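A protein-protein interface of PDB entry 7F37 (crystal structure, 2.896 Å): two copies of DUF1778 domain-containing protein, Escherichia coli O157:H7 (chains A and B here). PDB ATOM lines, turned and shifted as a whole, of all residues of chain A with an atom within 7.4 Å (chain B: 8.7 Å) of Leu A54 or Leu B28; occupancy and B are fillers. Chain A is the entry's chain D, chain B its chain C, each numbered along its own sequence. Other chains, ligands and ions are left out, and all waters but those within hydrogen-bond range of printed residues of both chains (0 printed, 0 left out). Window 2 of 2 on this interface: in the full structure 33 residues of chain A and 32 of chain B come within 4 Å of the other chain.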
ATOM      1  N   ALA A  45       3.099  15.137   1.521  1.00  0.00           N
ATOM      2  CA  ALA A  45       3.980  14.091   2.021  1.00  0.00           C
ATOM      3  C   ALA A  45       5.361  14.222   1.388  1.00  0.00           C
ATOM      4  O   ALA A  45       6.373  14.395   2.082  1.00  0.00           O
ATOM      5  CB  ALA A  45       3.363  12.717   1.733  1.00  0.00           C
ATOM      6  N   ILE A  48       7.285  17.104   2.569  1.00  0.00           N
ATOM      7  CA  ILE A  48       7.830  16.961   3.920  1.00  0.00           C
ATOM      8  C   ILE A  48       9.090  16.092   3.911  1.00  0.00           C
ATOM      9  O   ILE A  48      10.159  16.515   4.366  1.00  0.00           O
ATOM     10  CB  ILE A  48       6.766  16.418   4.885  1.00  0.00           C
ATOM     11  CG1 ILE A  48       5.875  17.564   5.360  1.00  0.00           C
ATOM     12  CG2 ILE A  48       7.413  15.733   6.056  1.00  0.00           C
ATOM     13  CD1 ILE A  48       4.571  17.087   5.935  1.00  0.00           C
ATOM     14  N   LEU A  49       8.996  14.877   3.363  1.00  0.00           N
ATOM     15  CA  LEU A  49      10.176  14.015   3.270  1.00  0.00           C
ATOM     16  C   LEU A  49      11.351  14.678   2.525  1.00  0.00           C
ATOM     17  O   LEU A  49      12.510  14.323   2.773  1.00  0.00           O
ATOM     18  CB  LEU A  49       9.788  12.675   2.622  1.00  0.00           C
ATOM     19  CG  LEU A  49       8.686  11.978   3.443  1.00  0.00           C
ATOM     20  CD1 LEU A  49       7.976  10.905   2.700  1.00  0.00           C
ATOM     21  CD2 LEU A  49       9.223  11.401   4.713  1.00  0.00           C
ATOM     22  N   LEU A  50      11.099  15.658   1.643  1.00  0.00           N
ATOM     23  CA  LEU A  50      12.175  16.302   0.878  1.00  0.00           C
ATOM     24  C   LEU A  50      12.692  17.584   1.527  1.00  0.00           C
ATOM     25  O   LEU A  50      13.359  18.387   0.859  1.00  0.00           O
ATOM     26  CB  LEU A  50      11.732  16.625  -0.553  1.00  0.00           C
ATOM     27  CG  LEU A  50      11.308  15.515  -1.499  1.00  0.00           C
ATOM     28  CD1 LEU A  50      11.037  16.107  -2.858  1.00  0.00           C
ATOM     29  CD2 LEU A  50      12.372  14.425  -1.552  1.00  0.00           C
ATOM     30  N   ASP A  51      12.394  17.800   2.797  1.00  0.00           N
ATOM     31  CA  ASP A  51      12.945  18.955   3.485  1.00  0.00           C
ATOM     32  C   ASP A  51      14.460  18.861   3.553  1.00  0.00           C
ATOM     33  O   ASP A  51      15.016  17.857   4.007  1.00  0.00           O
ATOM     34  CB  ASP A  51      12.358  19.064   4.885  1.00  0.00           C
ATOM     35  CG  ASP A  51      12.101  20.479   5.261  1.00  0.00           C
ATOM     36  OD1 ASP A  51      12.854  21.329   4.742  1.00  0.00           O
ATOM     37  OD2 ASP A  51      11.148  20.739   6.033  1.00  0.00           O
ATOM     38  N   GLN A  52      15.129  19.907   3.078  1.00  0.00           N
ATOM     39  CA  GLN A  52      16.565  20.025   3.301  1.00  0.00           C
ATOM     40  C   GLN A  52      16.899  20.165   4.778  1.00  0.00           C
ATOM     41  O   GLN A  52      18.078  20.071   5.140  1.00  0.00           O
ATOM     42  CB  GLN A  52      17.133  21.215   2.525  1.00  0.00           C
ATOM     43  CG  GLN A  52      16.325  21.618   1.284  1.00  0.00           C
ATOM     44  CD  GLN A  52      17.037  22.674   0.449  1.00  0.00           C
ATOM     45  OE1 GLN A  52      18.124  22.431  -0.085  1.00  0.00           O
ATOM     46  NE2 GLN A  52      16.433  23.862   0.349  1.00  0.00           N
ATOM     47  N   ARG A  53      15.886  20.401   5.629  1.00  0.00           N
ATOM     48  CA  ARG A  53      16.064  20.358   7.076  1.00  0.00           C
ATOM     49  C   ARG A  53      16.424  18.962   7.560  1.00  0.00           C
ATOM     50  O   ARG A  53      16.926  18.823   8.681  1.00  0.00           O
ATOM     51  CB  ARG A  53      14.794  20.837   7.796  1.00  0.00           C
ATOM     52  CG  ARG A  53      14.329  22.256   7.442  1.00  0.00           C
ATOM     53  CD  ARG A  53      15.348  23.310   7.905  1.00  0.00           C
ATOM     54  NE  ARG A  53      16.187  23.840   6.820  1.00  0.00           N
ATOM     55  CZ  ARG A  53      17.196  24.700   6.982  1.00  0.00           C
ATOM     56  NH1 ARG A  53      17.536  25.149   8.192  1.00  0.00           N
ATOM     57  NH2 ARG A  53      17.873  25.109   5.920  1.00  0.00           N
ATOM     58  N   LEU A  54      16.201  17.933   6.733  1.00  0.00           N
ATOM     59  CA  LEU A  54      16.477  16.545   7.099  1.00  0.00           C
ATOM     60  C   LEU A  54      17.898  16.080   6.764  1.00  0.00           C
ATOM     61  O   LEU A  54      18.244  14.928   7.058  1.00  0.00           O
ATOM     62  CB  LEU A  54      15.473  15.603   6.427  1.00  0.00           C
ATOM     63  CG  LEU A  54      13.972  15.798   6.577  1.00  0.00           C
ATOM     64  CD1 LEU A  54      13.363  14.472   6.149  1.00  0.00           C
ATOM     65  CD2 LEU A  54      13.565  16.211   8.006  1.00  0.00           C
ATOM     66  N   PHE A  55      18.730  16.921   6.153  1.00  0.00           N
ATOM     67  CA  PHE A  55      20.161  16.658   6.174  1.00  0.00           C
ATOM     68  C   PHE A  55      21.005  17.867   6.559  1.00  0.00           C
ATOM     69  O   PHE A  55      22.194  17.691   6.866  1.00  0.00           O
ATOM     70  CB  PHE A  55      20.651  16.095   4.825  1.00  0.00           C
ATOM     71  CG  PHE A  55      19.992  16.698   3.592  1.00  0.00           C
ATOM     72  CD1 PHE A  55      20.588  17.762   2.916  1.00  0.00           C
ATOM     73  CD2 PHE A  55      18.831  16.138   3.066  1.00  0.00           C
ATOM     74  CE1 PHE A  55      20.026  18.286   1.784  1.00  0.00           C
ATOM     75  CE2 PHE A  55      18.263  16.643   1.930  1.00  0.00           C
ATOM     76  CZ  PHE A  55      18.863  17.729   1.291  1.00  0.00           C
ATOM     77  N   ILE A  56      20.438  19.069   6.594  1.00  0.00           N
ATOM     78  CA  ILE A  56      21.183  20.279   6.924  1.00  0.00           C
ATOM     79  C   ILE A  56      20.822  20.682   8.355  1.00  0.00           C
ATOM     80  O   ILE A  56      19.837  21.392   8.593  1.00  0.00           O
ATOM     81  CB  ILE A  56      20.909  21.386   5.904  1.00  0.00           C
ATOM     82  CG1 ILE A  56      21.571  21.010   4.579  1.00  0.00           C
ATOM     83  CG2 ILE A  56      21.419  22.735   6.399  1.00  0.00           C
ATOM     84  CD1 ILE A  56      21.035  21.764   3.400  1.00  0.00           C
ATOM     85  N   LEU A  57      21.647  20.241   9.316  1.00  0.00           N
ATOM     86  CA  LEU A  57      21.344  20.321  10.742  1.00  0.00           C
ATOM     87  C   LEU A  57      21.723  21.665  11.370  1.00  0.00           C
ATOM     88  O   LEU A  57      21.879  21.737  12.596  1.00  0.00           O
ATOM     89  CB  LEU A  57      22.050  19.192  11.505  1.00  0.00           C
ATOM     90  CG  LEU A  57      21.813  17.722  11.142  1.00  0.00           C
ATOM     91  CD1 LEU A  57      20.343  17.476  10.765  1.00  0.00           C
ATOM     92  CD2 LEU A  57      22.809  17.214  10.060  1.00  0.00           C
ATOM     93  N   LEU B  21       3.464   6.227   1.457  1.00  0.00           N
ATOM     94  CA  LEU B  21       4.099   7.541   1.375  1.00  0.00           C
ATOM     95  C   LEU B  21       3.520   8.508   2.404  1.00  0.00           C
ATOM     96  O   LEU B  21       4.255   9.285   3.019  1.00  0.00           O
ATOM     97  CB  LEU B  21       3.958   8.103  -0.041  1.00  0.00           C
ATOM     98  CG  LEU B  21       4.198   9.605  -0.186  1.00  0.00           C
ATOM     99  CD1 LEU B  21       5.583   9.929   0.242  1.00  0.00           C
ATOM    100  CD2 LEU B  21       3.947  10.127  -1.602  1.00  0.00           C
ATOM    101  N   ILE B  22       2.208   8.462   2.620  1.00  0.00           N
ATOM    102  CA  ILE B  22       1.584   9.407   3.541  1.00  0.00           C
ATOM    103  C   ILE B  22       1.979   9.110   4.984  1.00  0.00           C
ATOM    104  O   ILE B  22       2.190  10.029   5.782  1.00  0.00           O
ATOM    105  CB  ILE B  22       0.061   9.390   3.350  1.00  0.00           C
ATOM    106  CG1 ILE B  22      -0.281   9.825   1.911  1.00  0.00           C
ATOM    107  CG2 ILE B  22      -0.564  10.273   4.369  1.00  0.00           C
ATOM    108  CD1 ILE B  22      -1.717   9.678   1.553  1.00  0.00           C
ATOM    109  N   ASP B  23       2.129   7.824   5.326  1.00  0.00           N
ATOM    110  CA  ASP B  23       2.409   7.427   6.706  1.00  0.00           C
ATOM    111  C   ASP B  23       3.770   7.914   7.184  1.00  0.00           C
ATOM    112  O   ASP B  23       3.891   8.487   8.278  1.00  0.00           O
ATOM    113  CB  ASP B  23       2.330   5.914   6.828  1.00  0.00           C
ATOM    114  CG  ASP B  23       0.968   5.407   6.535  1.00  0.00           C
ATOM    115  OD1 ASP B  23       0.239   6.132   5.827  1.00  0.00           O
ATOM    116  OD2 ASP B  23       0.618   4.310   7.024  1.00  0.00           O
ATOM    117  N   MET B  24       4.817   7.654   6.403  1.00  0.00           N
ATOM    118  CA  MET B  24       6.125   8.144   6.801  1.00  0.00           C
ATOM    119  C   MET B  24       6.100   9.653   6.965  1.00  0.00           C
ATOM    120  O   MET B  24       6.655  10.184   7.935  1.00  0.00           O
ATOM    121  CB  MET B  24       7.174   7.710   5.792  1.00  0.00           C
ATOM    122  CG  MET B  24       7.225   6.205   5.654  1.00  0.00           C
ATOM    123  SD  MET B  24       8.118   5.682   4.187  1.00  0.00           S
ATOM    124  CE  MET B  24       9.512   6.848   4.234  1.00  0.00           C
ATOM    125  N   ALA B  25       5.411  10.355   6.059  1.00  0.00           N
ATOM    126  CA  ALA B  25       5.293  11.800   6.188  1.00  0.00           C
ATOM    127  C   ALA B  25       4.611  12.172   7.490  1.00  0.00           C
ATOM    128  O   ALA B  25       5.136  12.978   8.275  1.00  0.00           O
ATOM    129  CB  ALA B  25       4.511  12.375   5.016  1.00  0.00           C
ATOM    130  N   ALA B  26       3.417  11.608   7.715  1.00  0.00           N
ATOM    131  CA  ALA B  26       2.680  11.819   8.949  1.00  0.00           C
ATOM    132  C   ALA B  26       3.600  11.698  10.160  1.00  0.00           C
ATOM    133  O   ALA B  26       3.706  12.619  10.981  1.00  0.00           O
ATOM    134  CB  ALA B  26       1.540  10.810   9.017  1.00  0.00           C
ATOM    135  N   ASN B  27       4.325  10.577  10.243  1.00  0.00           N
ATOM    136  CA  ASN B  27       5.204  10.332  11.381  1.00  0.00           C
ATOM    137  C   ASN B  27       6.169  11.479  11.624  1.00  0.00           C
ATOM    138  O   ASN B  27       6.517  11.771  12.767  1.00  0.00           O
ATOM    139  CB  ASN B  27       5.979   9.041  11.171  1.00  0.00           C
ATOM    140  CG  ASN B  27       6.155   8.285  12.452  1.00  0.00           C
ATOM    141  OD1 ASN B  27       5.178   8.029  13.169  1.00  0.00           O
ATOM    142  ND2 ASN B  27       7.401   7.953  12.783  1.00  0.00           N
ATOM    143  N   LEU B  28       6.624  12.134  10.567  1.00  0.00           N
ATOM    144  CA  LEU B  28       7.546  13.245  10.754  1.00  0.00           C
ATOM    145  C   LEU B  28       6.900  14.427  11.447  1.00  0.00           C
ATOM    146  O   LEU B  28       7.614  15.326  11.902  1.00  0.00           O
ATOM    147  CB  LEU B  28       8.088  13.724   9.415  1.00  0.00           C
ATOM    148  CG  LEU B  28       9.470  13.207   9.106  1.00  0.00           C
ATOM    149  CD1 LEU B  28       9.430  11.693   9.073  1.00  0.00           C
ATOM    150  CD2 LEU B  28       9.866  13.796   7.771  1.00  0.00           C
ATOM    151  N   VAL B  29       5.574  14.478  11.488  1.00  0.00           N
ATOM    152  CA  VAL B  29       4.906  15.694  11.920  1.00  0.00           C
ATOM    153  C   VAL B  29       3.877  15.364  12.993  1.00  0.00           C
ATOM    154  O   VAL B  29       2.986  16.171  13.297  1.00  0.00           O
ATOM    155  CB  VAL B  29       4.287  16.423  10.715  1.00  0.00           C
ATOM    156  CG1 VAL B  29       5.348  16.652   9.675  1.00  0.00           C
ATOM    157  CG2 VAL B  29       3.120  15.624  10.126  1.00  0.00           C
ATOM    158  N   ALA B  30       4.005  14.170  13.575  1.00  0.00           N
ATOM    159  CA  ALA B  30       3.209  13.753  14.733  1.00  0.00           C
ATOM    160  C   ALA B  30       1.708  13.767  14.444  1.00  0.00           C
ATOM    161  O   ALA B  30       0.905  14.187  15.279  1.00  0.00           O
ATOM    162  CB  ALA B  30       3.521  14.619  15.955  1.00  0.00           C
ATOM    163  N   LYS B  31       1.306  13.301  13.272  1.00  0.00           N
ATOM    164  CA  LYS B  31      -0.112  13.262  12.965  1.00  0.00           C
ATOM    165  C   LYS B  31      -0.535  11.847  12.604  1.00  0.00           C
ATOM    166  O   LYS B  31       0.224  11.080  12.011  1.00  0.00           O
ATOM    167  CB  LYS B  31      -0.484  14.219  11.816  1.00  0.00           C
ATOM    168  CG  LYS B  31       0.095  15.647  11.878  1.00  0.00           C
ATOM    169  CD  LYS B  31      -0.871  16.658  11.255  1.00  0.00           C
ATOM    170  CE  LYS B  31      -0.222  18.029  11.194  1.00  0.00           C
ATOM    171  NZ  LYS B  31      -1.095  19.036  10.526  1.00  0.00           N
ATOM    172  N   PHE B  36      -3.443  13.912   9.185  1.00  0.00           N
ATOM    173  CA  PHE B  36      -2.513  14.469   8.208  1.00  0.00           C
ATOM    174  C   PHE B  36      -3.210  14.748   6.889  1.00  0.00           C
ATOM    175  O   PHE B  36      -3.097  15.852   6.337  1.00  0.00           O
ATOM    176  CB  PHE B  36      -1.345  13.512   7.978  1.00  0.00           C
ATOM    177  CG  PHE B  36      -0.460  13.902   6.815  1.00  0.00           C
ATOM    178  CD1 PHE B  36       0.697  14.647   7.025  1.00  0.00           C
ATOM    179  CD2 PHE B  36      -0.775  13.515   5.518  1.00  0.00           C
ATOM    180  CE1 PHE B  36       1.511  15.000   5.962  1.00  0.00           C
ATOM    181  CE2 PHE B  36       0.020  13.873   4.462  1.00  0.00           C
ATOM    182  CZ  PHE B  36       1.161  14.613   4.684  1.00  0.00           C
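Hydrophobic or aromatic side chains of chain B that line the printed part of chain A: Leu B21, Ala B25, Leu B28, Val B29 and Phe B36. Hydrophobic or aromatic side chains of chain A within 4 Å of the printed part of chain B: Ala A45, Ile A48, Leu A49 and Leu A54. Among the printed residues, 9 pairs touch across the chains.
No position is printed for both chains. Of the 9 pairs that touch across the chains among the printed residues, none has its exchanged pair printed and touching as well.
Of chain B, only Leu B28 comes within 4 Å of Leu A54. Printed residues of chain A within 4 Å of Val B29: Ile A48. Of the printed residues of chain A, Phe B36 touches Ala A45 (3.7 Å) and Ile A48 (3.7 Å). Of the printed residues of chain B, Ile A48 touches Leu B28 (3.6 Å), Val B29 (3.8 Å) and Phe B36 (3.7 Å). Of the printed residues of chain B, Leu A49 touches Leu B21 (3.6 Å) and Leu B28 (3.9 Å). Asn B27 touches none of the printed residues of chain A. Met B24 touches none of the printed residues of chain A.
Among the printed residues, merely in contact across the chains: Ala A45 with Ala B25, Ile A48 with Leu B28, Leu A49 with Leu B21, Ile A48 with Phe B36, Ala A45 with Phe B36, Ala A45 with Leu B21, Ile A48 with Val B29, Leu A54 with Leu B28 and Leu A49 with Leu B28.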
